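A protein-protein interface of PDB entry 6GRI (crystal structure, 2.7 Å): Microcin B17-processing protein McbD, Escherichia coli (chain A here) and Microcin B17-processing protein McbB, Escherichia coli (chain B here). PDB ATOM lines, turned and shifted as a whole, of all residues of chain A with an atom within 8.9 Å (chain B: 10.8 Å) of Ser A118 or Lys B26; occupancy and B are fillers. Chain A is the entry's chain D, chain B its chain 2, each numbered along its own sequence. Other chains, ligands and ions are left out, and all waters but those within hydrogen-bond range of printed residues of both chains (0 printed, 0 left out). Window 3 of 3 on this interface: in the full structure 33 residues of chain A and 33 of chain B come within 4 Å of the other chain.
The backbone carbonyl oxygen of Leu A116 lies within hydrogen-bond range of the guanidinium group of Arg B23, 2.5 Å away. OD1 of Asp B37 sits at hydrogen-bond distance from NE2 of Gln A121 (3.1 Å).
N of Leu A116 sits at hydrogen-bond distance from O of Ile A338 (2.9 Å). OG of Ser A118 lies within hydrogen-bond range of N of Glu A120 (3.1 Å). O of Ile B21 sits at hydrogen-bond distance from N of Leu B28 (2.7 Å). N of Val A340 sits at hydrogen-bond distance from O of Phe A114 (2.7 Å). The side-chain hydroxyl (OG) of Ser B22 is in hydrogen-bond range of the backbone carbonyl oxygen (O) of Lys B26. The side-chain amide oxygen (OD1) of Asn A115 lies within hydrogen-bond range of the backbone NH (N) of Phe A117 (2.9 Å).
Leu B28 touches Phe A114. CG of Arg B23 touches O of Phe A117, at 3.6 Å. O of Ser A118 touches CB of Lys B26 (3.6 Å). Ile B21 touches Leu A119. Leu A119 touches Ser B22 (CD1 to CA, 3.9 Å). Leu A119 touches Arg B23 (CD1 to N, 3.9 Å). CD1 of Leu A119 touches O of Lys B26, at 3.7 Å. OD1 of Asp B37 touches O of Leu A119, 3.97 Å away. Leu B28 touches Gln A121. Arg B23 touches Leu A328 (NH1 to CD1, 3.7 Å).
Ser A118 touches one residue of chain B. Lys B26 touches two residues of chain A. No residue of chain B comes within 4 Å of Asn A115. Leu A119 touches five residues of chain B. No residue of chain A comes within 4 Å of Thr B25. No residue of chain A comes within 4 Å of Thr B27. Printed residues of chain B within 4 Å of Phe A114: Leu B28 (3.9 Å). Of the printed residues of chain B, Phe A117 touches Arg B23 (3.6 Å). Of the printed residues of chain B, Leu A116 touches Arg B23. Of the printed residues of chain A, Asp B37 touches Leu A119 and Gln A121. Met B43 touches none of the printed residues of chain A. Phe A339 touches none of the printed residues of chain B. The nearest residue of chain A that does not touch Lys B26 is Glu A120 (6.2 Å).
Printed residues of chain A that touch a printed residue of chain B: Phe A114, Leu A116, Phe A117, Ser A118, Leu A119, Gln A121 and Leu A328. Hydrophobic or aromatic side chains of chain A that line the printed part of chain B: Phe A114, Leu A116, Leu A119 and Leu A328. Of the 21 printed residues of chain B, 6 touch a printed residue of chain A. Hydrophobic or aromatic side chains of chain B that line the printed part of chain A: Leu B28. Along chain B the printed residues that touch a printed residue of chain A span positions 21 to 37. Among the printed residues, 12 pairs touch across the chains.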
ATOM      1  N   PRO A  81      25.930  -8.273 -34.756  1.00  0.00           N
ATOM      2  CA  PRO A  81      27.028  -8.800 -35.567  1.00  0.00           C
ATOM      3  C   PRO A  81      27.008  -8.256 -37.001  1.00  0.00           C
ATOM      4  O   PRO A  81      25.981  -7.707 -37.426  1.00  0.00           O
ATOM      5  CB  PRO A  81      26.781 -10.315 -35.555  1.00  0.00           C
ATOM      6  CG  PRO A  81      25.967 -10.559 -34.334  1.00  0.00           C
ATOM      7  CD  PRO A  81      25.070  -9.365 -34.261  1.00  0.00           C
ATOM      8  N   PHE A 114      17.095 -11.549 -29.616  1.00  0.00           N
ATOM      9  CA  PHE A 114      17.974 -12.705 -29.743  1.00  0.00           C
ATOM     10  C   PHE A 114      17.723 -13.385 -31.072  1.00  0.00           C
ATOM     11  O   PHE A 114      16.623 -13.284 -31.628  1.00  0.00           O
ATOM     12  CB  PHE A 114      17.845 -13.675 -28.548  1.00  0.00           C
ATOM     13  CG  PHE A 114      16.492 -14.340 -28.405  1.00  0.00           C
ATOM     14  CD1 PHE A 114      16.232 -15.566 -29.009  1.00  0.00           C
ATOM     15  CD2 PHE A 114      15.502 -13.766 -27.620  1.00  0.00           C
ATOM     16  CE1 PHE A 114      15.006 -16.192 -28.849  1.00  0.00           C
ATOM     17  CE2 PHE A 114      14.267 -14.384 -27.457  1.00  0.00           C
ATOM     18  CZ  PHE A 114      14.019 -15.601 -28.070  1.00  0.00           C
ATOM     19  N   ASN A 115      18.761 -14.042 -31.584  1.00  0.00           N
ATOM     20  CA  ASN A 115      18.698 -14.738 -32.871  1.00  0.00           C
ATOM     21  C   ASN A 115      17.844 -15.992 -32.727  1.00  0.00           C
ATOM     22  O   ASN A 115      18.087 -16.824 -31.844  1.00  0.00           O
ATOM     23  CB  ASN A 115      20.106 -15.102 -33.372  1.00  0.00           C
ATOM     24  CG  ASN A 115      20.092 -15.750 -34.744  1.00  0.00           C
ATOM     25  OD1 ASN A 115      19.924 -16.964 -34.873  1.00  0.00           O
ATOM     26  ND2 ASN A 115      20.257 -14.940 -35.777  1.00  0.00           N
ATOM     27  N   LEU A 116      16.858 -16.122 -33.609  1.00  0.00           N
ATOM     28  CA  LEU A 116      15.900 -17.230 -33.570  1.00  0.00           C
ATOM     29  C   LEU A 116      16.602 -18.581 -33.553  1.00  0.00           C
ATOM     30  O   LEU A 116      16.134 -19.502 -32.901  1.00  0.00           O
ATOM     31  CB  LEU A 116      14.956 -17.156 -34.780  1.00  0.00           C
ATOM     32  CG  LEU A 116      13.773 -18.125 -34.884  1.00  0.00           C
ATOM     33  CD1 LEU A 116      12.751 -17.852 -33.792  1.00  0.00           C
ATOM     34  CD2 LEU A 116      13.114 -18.030 -36.255  1.00  0.00           C
ATOM     35  N   PHE A 117      17.734 -18.688 -34.247  1.00  0.00           N
ATOM     36  CA  PHE A 117      18.396 -19.977 -34.453  1.00  0.00           C
ATOM     37  C   PHE A 117      19.504 -20.269 -33.438  1.00  0.00           C
ATOM     38  O   PHE A 117      19.521 -21.336 -32.832  1.00  0.00           O
ATOM     39  CB  PHE A 117      18.913 -20.053 -35.895  1.00  0.00           C
ATOM     40  CG  PHE A 117      17.859 -19.720 -36.920  1.00  0.00           C
ATOM     41  CD1 PHE A 117      16.714 -20.504 -37.037  1.00  0.00           C
ATOM     42  CD2 PHE A 117      17.984 -18.605 -37.745  1.00  0.00           C
ATOM     43  CE1 PHE A 117      15.723 -20.195 -37.959  1.00  0.00           C
ATOM     44  CE2 PHE A 117      16.998 -18.300 -38.683  1.00  0.00           C
ATOM     45  CZ  PHE A 117      15.866 -19.096 -38.788  1.00  0.00           C
ATOM     46  N   SER A 118      20.407 -19.315 -33.240  1.00  0.00           N
ATOM     47  CA  SER A 118      21.590 -19.520 -32.406  1.00  0.00           C
ATOM     48  C   SER A 118      21.399 -19.126 -30.954  1.00  0.00           C
ATOM     49  O   SER A 118      22.254 -19.434 -30.123  1.00  0.00           O
ATOM     50  CB  SER A 118      22.759 -18.711 -32.966  1.00  0.00           C
ATOM     51  OG  SER A 118      22.625 -17.333 -32.655  1.00  0.00           O
ATOM     52  N   LEU A 119      20.313 -18.401 -30.671  1.00  0.00           N
ATOM     53  CA  LEU A 119      20.079 -17.753 -29.380  1.00  0.00           C
ATOM     54  C   LEU A 119      21.126 -16.706 -28.946  1.00  0.00           C
ATOM     55  O   LEU A 119      21.161 -16.334 -27.771  1.00  0.00           O
ATOM     56  CB  LEU A 119      19.894 -18.808 -28.287  1.00  0.00           C
ATOM     57  CG  LEU A 119      18.899 -19.934 -28.578  1.00  0.00           C
ATOM     58  CD1 LEU A 119      18.609 -20.695 -27.296  1.00  0.00           C
ATOM     59  CD2 LEU A 119      17.602 -19.413 -29.175  1.00  0.00           C
ATOM     60  N   GLU A 120      21.950 -16.208 -29.878  1.00  0.00           N
ATOM     61  CA  GLU A 120      22.887 -15.129 -29.566  1.00  0.00           C
ATOM     62  C   GLU A 120      22.082 -13.861 -29.320  1.00  0.00           C
ATOM     63  O   GLU A 120      21.142 -13.553 -30.058  1.00  0.00           O
ATOM     64  CB  GLU A 120      23.911 -14.891 -30.691  1.00  0.00           C
ATOM     65  CG  GLU A 120      24.766 -13.626 -30.510  1.00  0.00           C
ATOM     66  CD  GLU A 120      25.944 -13.528 -31.475  1.00  0.00           C
ATOM     67  OE1 GLU A 120      25.738 -13.687 -32.700  1.00  0.00           O
ATOM     68  OE2 GLU A 120      27.080 -13.273 -31.008  1.00  0.00           O
ATOM     69  N   GLN A 121      22.472 -13.128 -28.285  1.00  0.00           N
ATOM     70  CA  GLN A 121      21.787 -11.904 -27.900  1.00  0.00           C
ATOM     71  C   GLN A 121      22.439 -10.740 -28.615  1.00  0.00           C
ATOM     72  O   GLN A 121      23.656 -10.697 -28.757  1.00  0.00           O
ATOM     73  CB  GLN A 121      21.876 -11.692 -26.399  1.00  0.00           C
ATOM     74  CG  GLN A 121      21.437 -12.887 -25.584  1.00  0.00           C
ATOM     75  CD  GLN A 121      21.568 -12.624 -24.107  1.00  0.00           C
ATOM     76  OE1 GLN A 121      20.828 -11.814 -23.546  1.00  0.00           O
ATOM     77  NE2 GLN A 121      22.518 -13.300 -23.467  1.00  0.00           N
ATOM     78  N   GLN A 122      21.618  -9.800 -29.061  1.00  0.00           N
ATOM     79  CA  GLN A 122      22.084  -8.591 -29.730  1.00  0.00           C
ATOM     80  C   GLN A 122      20.987  -7.546 -29.596  1.00  0.00           C
ATOM     81  O   GLN A 122      20.017  -7.757 -28.866  1.00  0.00           O
ATOM     82  CB  GLN A 122      22.397  -8.897 -31.193  1.00  0.00           C
ATOM     83  CG  GLN A 122      21.339  -9.743 -31.888  1.00  0.00           C
ATOM     84  CD  GLN A 122      21.579  -9.849 -33.380  1.00  0.00           C
ATOM     85  OE1 GLN A 122      21.165  -8.975 -34.145  1.00  0.00           O
ATOM     86  NE2 GLN A 122      22.245 -10.925 -33.801  1.00  0.00           N
ATOM     87  N   LEU A 328      11.962 -24.050 -38.352  1.00  0.00           N
ATOM     88  CA  LEU A 328      13.196 -23.291 -38.117  1.00  0.00           C
ATOM     89  C   LEU A 328      14.299 -23.675 -39.103  1.00  0.00           C
ATOM     90  O   LEU A 328      15.047 -22.810 -39.576  1.00  0.00           O
ATOM     91  CB  LEU A 328      13.681 -23.473 -36.674  1.00  0.00           C
ATOM     92  CG  LEU A 328      12.706 -23.090 -35.551  1.00  0.00           C
ATOM     93  CD1 LEU A 328      13.460 -22.934 -34.237  1.00  0.00           C
ATOM     94  CD2 LEU A 328      11.937 -21.816 -35.867  1.00  0.00           C
ATOM     95  N   GLN A 332      15.835 -21.048 -41.667  1.00  0.00           N
ATOM     96  CA  GLN A 332      17.293 -20.809 -41.602  1.00  0.00           C
ATOM     97  C   GLN A 332      17.978 -21.009 -42.951  1.00  0.00           C
ATOM     98  O   GLN A 332      18.875 -20.247 -43.292  1.00  0.00           O
ATOM     99  CB  GLN A 332      17.979 -21.669 -40.532  1.00  0.00           C
ATOM    100  CG  GLN A 332      19.483 -21.404 -40.412  1.00  0.00           C
ATOM    101  CD  GLN A 332      20.094 -21.895 -39.105  1.00  0.00           C
ATOM    102  OE1 GLN A 332      19.587 -22.828 -38.473  1.00  0.00           O
ATOM    103  NE2 GLN A 332      21.194 -21.264 -38.695  1.00  0.00           N
ATOM    104  N   ASP A 336      19.768 -16.595 -42.047  1.00  0.00           N
ATOM    105  CA  ASP A 336      20.281 -16.706 -40.679  1.00  0.00           C
ATOM    106  C   ASP A 336      19.788 -15.524 -39.826  1.00  0.00           C
ATOM    107  O   ASP A 336      19.612 -15.666 -38.611  1.00  0.00           O
ATOM    108  CB  ASP A 336      21.827 -16.728 -40.715  1.00  0.00           C
ATOM    109  CG  ASP A 336      22.433 -17.675 -39.699  1.00  0.00           C
ATOM    110  OD1 ASP A 336      22.425 -17.343 -38.493  1.00  0.00           O
ATOM    111  OD2 ASP A 336      22.945 -18.745 -40.116  1.00  0.00           O
ATOM    112  N   ASN A 337      19.561 -14.377 -40.477  1.00  0.00           N
ATOM    113  CA  ASN A 337      19.228 -13.118 -39.804  1.00  0.00           C
ATOM    114  C   ASN A 337      17.717 -12.991 -39.532  1.00  0.00           C
ATOM    115  O   ASN A 337      17.016 -12.234 -40.211  1.00  0.00           O
ATOM    116  CB  ASN A 337      19.701 -11.924 -40.651  1.00  0.00           C
ATOM    117  CG  ASN A 337      21.192 -11.969 -40.981  1.00  0.00           C
ATOM    118  OD1 ASN A 337      22.042 -12.105 -40.101  1.00  0.00           O
ATOM    119  ND2 ASN A 337      21.510 -11.830 -42.263  1.00  0.00           N
ATOM    120  N   ILE A 338      17.227 -13.752 -38.550  1.00  0.00           N
ATOM    121  CA  ILE A 338      15.831 -13.662 -38.067  1.00  0.00           C
ATOM    122  C   ILE A 338      15.895 -13.508 -36.548  1.00  0.00           C
ATOM    123  O   ILE A 338      16.371 -14.408 -35.847  1.00  0.00           O
ATOM    124  CB  ILE A 338      14.974 -14.900 -38.424  1.00  0.00           C
ATOM    125  CG1 ILE A 338      15.112 -15.247 -39.903  1.00  0.00           C
ATOM    126  CG2 ILE A 338      13.508 -14.645 -38.116  1.00  0.00           C
ATOM    127  CD1 ILE A 338      14.189 -16.359 -40.362  1.00  0.00           C
ATOM    128  N   PHE A 339      15.399 -12.374 -36.055  1.00  0.00           N
ATOM    129  CA  PHE A 339      15.578 -11.963 -34.661  1.00  0.00           C
ATOM    130  C   PHE A 339      14.242 -11.928 -33.931  1.00  0.00           C
ATOM    131  O   PHE A 339      13.198 -11.611 -34.517  1.00  0.00           O
ATOM    132  CB  PHE A 339      16.289 -10.608 -34.617  1.00  0.00           C
ATOM    133  CG  PHE A 339      17.444 -10.541 -35.556  1.00  0.00           C
ATOM    134  CD1 PHE A 339      18.695 -10.995 -35.171  1.00  0.00           C
ATOM    135  CD2 PHE A 339      17.260 -10.111 -36.870  1.00  0.00           C
ATOM    136  CE1 PHE A 339      19.753 -10.982 -36.066  1.00  0.00           C
ATOM    137  CE2 PHE A 339      18.311 -10.097 -37.764  1.00  0.00           C
ATOM    138  CZ  PHE A 339      19.558 -10.530 -37.361  1.00  0.00           C
ATOM    139  N   VAL A 340      14.288 -12.297 -32.654  1.00  0.00           N
ATOM    140  CA  VAL A 340      13.134 -12.228 -31.784  1.00  0.00           C
ATOM    141  C   VAL A 340      13.342 -11.080 -30.813  1.00  0.00           C
ATOM    142  O   VAL A 340      14.129 -11.197 -29.874  1.00  0.00           O
ATOM    143  CB  VAL A 340      12.949 -13.516 -30.964  1.00  0.00           C
ATOM    144  CG1 VAL A 340      11.679 -13.406 -30.109  1.00  0.00           C
ATOM    145  CG2 VAL A 340      12.930 -14.737 -31.870  1.00  0.00           C
ATOM    146  N   GLU B  19      11.979 -18.527 -17.974  1.00  0.00           N
ATOM    147  CA  GLU B  19      11.926 -19.329 -19.190  1.00  0.00           C
ATOM    148  C   GLU B  19      13.339 -19.713 -19.604  1.00  0.00           C
ATOM    149  O   GLU B  19      14.308 -19.023 -19.254  1.00  0.00           O
ATOM    150  CB  GLU B  19      11.260 -18.533 -20.321  1.00  0.00           C
ATOM    151  CG  GLU B  19       9.813 -18.119 -20.057  1.00  0.00           C
ATOM    152  CD  GLU B  19       8.779 -19.219 -20.257  1.00  0.00           C
ATOM    153  OE1 GLU B  19       9.106 -20.325 -20.749  1.00  0.00           O
ATOM    154  OE2 GLU B  19       7.604 -18.954 -19.936  1.00  0.00           O
ATOM    155  N   ILE B  20      13.441 -20.815 -20.350  1.00  0.00           N
ATOM    156  CA  ILE B  20      14.705 -21.283 -20.939  1.00  0.00           C
ATOM    157  C   ILE B  20      14.496 -21.757 -22.390  1.00  0.00           C
ATOM    158  O   ILE B  20      14.017 -22.866 -22.628  1.00  0.00           O
ATOM    159  CB  ILE B  20      15.418 -22.384 -20.088  1.00  0.00           C
ATOM    160  CG1 ILE B  20      14.402 -23.267 -19.336  1.00  0.00           C
ATOM    161  CG2 ILE B  20      16.419 -21.758 -19.115  1.00  0.00           C
ATOM    162  CD1 ILE B  20      15.002 -24.259 -18.356  1.00  0.00           C
ATOM    163  N   ILE B  21      14.817 -20.878 -23.344  1.00  0.00           N
ATOM    164  CA  ILE B  21      14.911 -21.220 -24.763  1.00  0.00           C
ATOM    165  C   ILE B  21      16.215 -21.990 -24.945  1.00  0.00           C
ATOM    166  O   ILE B  21      17.273 -21.511 -24.537  1.00  0.00           O
ATOM    167  CB  ILE B  21      14.951 -19.956 -25.642  1.00  0.00           C
ATOM    168  N   SER B  22      16.147 -23.186 -25.521  1.00  0.00           N
ATOM    169  CA  SER B  22      17.348 -24.010 -25.726  1.00  0.00           C
ATOM    170  C   SER B  22      17.281 -24.718 -27.082  1.00  0.00           C
ATOM    171  O   SER B  22      16.305 -25.420 -27.368  1.00  0.00           O
ATOM    172  CB  SER B  22      17.507 -25.009 -24.580  1.00  0.00           C
ATOM    173  OG  SER B  22      18.867 -25.362 -24.401  1.00  0.00           O
ATOM    174  N   ARG B  23      18.321 -24.535 -27.906  1.00  0.00           N
ATOM    175  CA  ARG B  23      18.247 -24.852 -29.338  1.00  0.00           C
ATOM    176  C   ARG B  23      19.494 -25.637 -29.820  1.00  0.00           C
ATOM    177  O   ARG B  23      19.768 -26.718 -29.277  1.00  0.00           O
ATOM    178  CB  ARG B  23      17.942 -23.552 -30.114  1.00  0.00           C
ATOM    179  CG  ARG B  23      17.224 -23.735 -31.449  1.00  0.00           C
ATOM    180  CD  ARG B  23      16.271 -22.579 -31.746  1.00  0.00           C
ATOM    181  NE  ARG B  23      15.166 -22.520 -30.785  1.00  0.00           N
ATOM    182  CZ  ARG B  23      14.255 -21.542 -30.701  1.00  0.00           C
ATOM    183  NH1 ARG B  23      14.271 -20.503 -31.532  1.00  0.00           N
ATOM    184  NH2 ARG B  23      13.305 -21.605 -29.766  1.00  0.00           N
ATOM    185  N   ASN B  24      20.231 -25.137 -30.816  1.00  0.00           N
ATOM    186  CA  ASN B  24      21.381 -25.858 -31.381  1.00  0.00           C
ATOM    187  C   ASN B  24      22.639 -25.767 -30.489  1.00  0.00           C
ATOM    188  O   ASN B  24      23.577 -25.021 -30.805  1.00  0.00           O
ATOM    189  CB  ASN B  24      21.679 -25.325 -32.789  1.00  0.00           C
ATOM    190  N   THR B  25      22.636 -26.527 -29.383  1.00  0.00           N
ATOM    191  CA  THR B  25      23.731 -26.568 -28.375  1.00  0.00           C
ATOM    192  C   THR B  25      23.679 -25.443 -27.312  1.00  0.00           C
ATOM    193  O   THR B  25      24.170 -25.633 -26.189  1.00  0.00           O
ATOM    194  CB  THR B  25      25.148 -26.603 -29.014  1.00  0.00           C
ATOM    195  N   LYS B  26      23.085 -24.293 -27.654  1.00  0.00           N
ATOM    196  CA  LYS B  26      23.092 -23.107 -26.794  1.00  0.00           C
ATOM    197  C   LYS B  26      21.807 -23.055 -25.971  1.00  0.00           C
ATOM    198  O   LYS B  26      20.767 -23.567 -26.407  1.00  0.00           O
ATOM    199  CB  LYS B  26      23.251 -21.844 -27.648  1.00  0.00           C
ATOM    200  N   THR B  27      21.892 -22.447 -24.784  1.00  0.00           N
ATOM    201  CA  THR B  27      20.761 -22.372 -23.840  1.00  0.00           C
ATOM    202  C   THR B  27      20.623 -20.972 -23.202  1.00  0.00           C
ATOM    203  O   THR B  27      21.575 -20.458 -22.619  1.00  0.00           O
ATOM    204  CB  THR B  27      20.906 -23.432 -22.728  1.00  0.00           C
ATOM    205  OG1 THR B  27      21.264 -24.691 -23.306  1.00  0.00           O
ATOM    206  CG2 THR B  27      19.605 -23.592 -21.939  1.00  0.00           C
ATOM    207  N   LEU B  28      19.431 -20.373 -23.305  1.00  0.00           N
ATOM    208  CA  LEU B  28      19.189 -18.990 -22.862  1.00  0.00           C
ATOM    209  C   LEU B  28      18.255 -18.941 -21.644  1.00  0.00           C
ATOM    210  O   LEU B  28      17.120 -19.393 -21.720  1.00  0.00           O
ATOM    211  CB  LEU B  28      18.599 -18.170 -24.019  1.00  0.00           C
ATOM    212  CG  LEU B  28      18.408 -16.658 -23.843  1.00  0.00           C
ATOM    213  CD1 LEU B  28      19.707 -15.955 -23.492  1.00  0.00           C
ATOM    214  CD2 LEU B  28      17.819 -16.046 -25.104  1.00  0.00           C
ATOM    215  N   LEU B  29      18.745 -18.404 -20.527  1.00  0.00           N
ATOM    216  CA  LEU B  29      17.925 -18.143 -19.339  1.00  0.00           C
ATOM    217  C   LEU B  29      17.415 -16.708 -19.385  1.00  0.00           C
ATOM    218  O   LEU B  29      18.225 -15.777 -19.422  1.00  0.00           O
ATOM    219  CB  LEU B  29      18.748 -18.352 -18.056  1.00  0.00           C
ATOM    220  CG  LEU B  29      18.190 -17.817 -16.724  1.00  0.00           C
ATOM    221  CD1 LEU B  29      16.871 -18.493 -16.387  1.00  0.00           C
ATOM    222  CD2 LEU B  29      19.203 -18.021 -15.608  1.00  0.00           C
ATOM    223  N   VAL B  36      20.706 -14.510 -19.788  1.00  0.00           N
ATOM    224  CA  VAL B  36      21.993 -15.189 -19.592  1.00  0.00           C
ATOM    225  C   VAL B  36      22.231 -16.371 -20.545  1.00  0.00           C
ATOM    226  O   VAL B  36      21.360 -17.218 -20.740  1.00  0.00           O
ATOM    227  CB  VAL B  36      22.144 -15.660 -18.125  1.00  0.00           C
ATOM    228  CG1 VAL B  36      23.477 -16.382 -17.909  1.00  0.00           C
ATOM    229  CG2 VAL B  36      22.002 -14.474 -17.176  1.00  0.00           C
ATOM    230  N   ASP B  37      23.438 -16.427 -21.109  1.00  0.00           N
ATOM    231  CA  ASP B  37      23.859 -17.549 -21.944  1.00  0.00           C
ATOM    232  C   ASP B  37      24.386 -18.642 -21.011  1.00  0.00           C
ATOM    233  O   ASP B  37      25.447 -18.503 -20.408  1.00  0.00           O
ATOM    234  CB  ASP B  37      24.917 -17.109 -22.965  1.00  0.00           C
ATOM    235  CG  ASP B  37      24.448 -15.930 -23.831  1.00  0.00           C
ATOM    236  OD1 ASP B  37      23.392 -16.053 -24.503  1.00  0.00           O
ATOM    237  OD2 ASP B  37      25.138 -14.880 -23.831  1.00  0.00           O
ATOM    238  N   ILE B  38      23.606 -19.712 -20.878  1.00  0.00           N
ATOM    239  CA  ILE B  38      23.912 -20.817 -19.977  1.00  0.00           C
ATOM    240  C   ILE B  38      24.950 -21.726 -20.649  1.00  0.00           C
ATOM    241  O   ILE B  38      24.640 -22.493 -21.561  1.00  0.00           O
ATOM    242  CB  ILE B  38      22.622 -21.590 -19.589  1.00  0.00           C
ATOM    243  CG1 ILE B  38      21.624 -20.669 -18.866  1.00  0.00           C
ATOM    244  CG2 ILE B  38      22.933 -22.814 -18.731  1.00  0.00           C
ATOM    245  CD1 ILE B  38      22.080 -20.148 -17.514  1.00  0.00           C
ATOM    246  N   THR B  39      26.189 -21.613 -20.188  1.00  0.00           N
ATOM    247  CA  THR B  39      27.319 -22.302 -20.798  1.00  0.00           C
ATOM    248  C   THR B  39      27.375 -23.751 -20.340  1.00  0.00           C
ATOM    249  O   THR B  39      27.284 -24.666 -21.163  1.00  0.00           O
ATOM    250  CB  THR B  39      28.636 -21.587 -20.444  1.00  0.00           C
ATOM    251  OG1 THR B  39      28.622 -20.285 -21.031  1.00  0.00           O
ATOM    252  CG2 THR B  39      29.854 -22.353 -20.947  1.00  0.00           C
ATOM    253  N   HIS B  40      27.518 -23.947 -19.028  1.00  0.00           N
ATOM    254  CA  HIS B  40      27.774 -25.271 -18.453  1.00  0.00           C
ATOM    255  C   HIS B  40      26.503 -26.125 -18.453  1.00  0.00           C
ATOM    256  O   HIS B  40      25.432 -25.638 -18.113  1.00  0.00           O
ATOM    257  CB  HIS B  40      28.369 -25.137 -17.043  1.00  0.00           C
ATOM    258  CG  HIS B  40      29.704 -24.451 -17.015  1.00  0.00           C
ATOM    259  ND1 HIS B  40      29.837 -23.078 -17.018  1.00  0.00           N
ATOM    260  CD2 HIS B  40      30.965 -24.950 -16.992  1.00  0.00           C
ATOM    261  CE1 HIS B  40      31.120 -22.761 -16.992  1.00  0.00           C
ATOM    262  NE2 HIS B  40      31.824 -23.878 -16.974  1.00  0.00           N
ATOM    263  N   GLU B  41      26.640 -27.394 -18.844  1.00  0.00           N
ATOM    264  CA  GLU B  41      25.498 -28.293 -19.090  1.00  0.00           C
ATOM    265  C   GLU B  41      24.765 -28.760 -17.824  1.00  0.00           C
ATOM    266  O   GLU B  41      23.573 -29.074 -17.881  1.00  0.00           O
ATOM    267  CB  GLU B  41      25.945 -29.517 -19.900  1.00  0.00           C
ATOM    268  N   MET B  43      24.258 -26.834 -15.209  1.00  0.00           N
ATOM    269  CA  MET B  43      23.375 -25.693 -14.940  1.00  0.00           C
ATOM    270  C   MET B  43      22.102 -25.724 -15.790  1.00  0.00           C
ATOM    271  O   MET B  43      21.054 -25.233 -15.355  1.00  0.00           O
ATOM    272  CB  MET B  43      24.106 -24.358 -15.159  1.00  0.00           C
ATOM    273  CG  MET B  43      24.290 -23.546 -13.895  1.00  0.00           C
ATOM    274  SD  MET B  43      22.715 -22.886 -13.328  1.00  0.00           S
ATOM    275  CE  MET B  43      23.083 -22.690 -11.586  1.00  0.00           C
ATOM    276  N   LYS B  44      22.205 -26.260 -17.010  1.00  0.00           N
ATOM    277  CA  LYS B  44      21.025 -26.560 -17.827  1.00  0.00           C
ATOM    278  C   LYS B  44      20.093 -27.544 -17.096  1.00  0.00           C
ATOM    279  O   LYS B  44      18.877 -27.339 -17.085  1.00  0.00           O
ATOM    280  CB  LYS B  44      21.431 -27.105 -19.204  1.00  0.00           C
ATOM    281  N   LEU B  47      18.650 -25.692 -13.934  1.00  0.00           N
ATOM    282  CA  LEU B  47      17.574 -24.814 -14.422  1.00  0.00           C
ATOM    283  C   LEU B  47      16.392 -25.570 -15.046  1.00  0.00           C
ATOM    284  O   LEU B  47      15.260 -25.095 -14.958  1.00  0.00           O
ATOM    285  CB  LEU B  47      18.118 -23.767 -15.401  1.00  0.00           C
ATOM    286  CG  LEU B  47      19.018 -22.672 -14.809  1.00  0.00           C
ATOM    287  CD1 LEU B  47      19.707 -21.905 -15.922  1.00  0.00           C
ATOM    288  CD2 LEU B  47      18.247 -21.707 -13.918  1.00  0.00           C
ATOM    289  N   GLU B  48      16.645 -26.730 -15.659  1.00  0.00           N
ATOM    290  CA  GLU B  48      15.560 -27.596 -16.166  1.00  0.00           C
ATOM    291  C   GLU B  48      14.666 -28.033 -15.005  1.00  0.00           C
ATOM    292  O   GLU B  48      13.450 -27.828 -15.031  1.00  0.00           O
ATOM    293  CB  GLU B  48      16.099 -28.854 -16.881  1.00  0.00           C
ATOM    294  CG  GLU B  48      15.550 -29.076 -18.285  1.00  0.00           C
ATOM    295  CD  GLU B  48      16.460 -28.515 -19.369  1.00  0.00           C
ATOM    296  OE1 GLU B  48      17.450 -29.194 -19.729  1.00  0.00           O
ATOM    297  OE2 GLU B  48      16.179 -27.402 -19.870  1.00  0.00           O
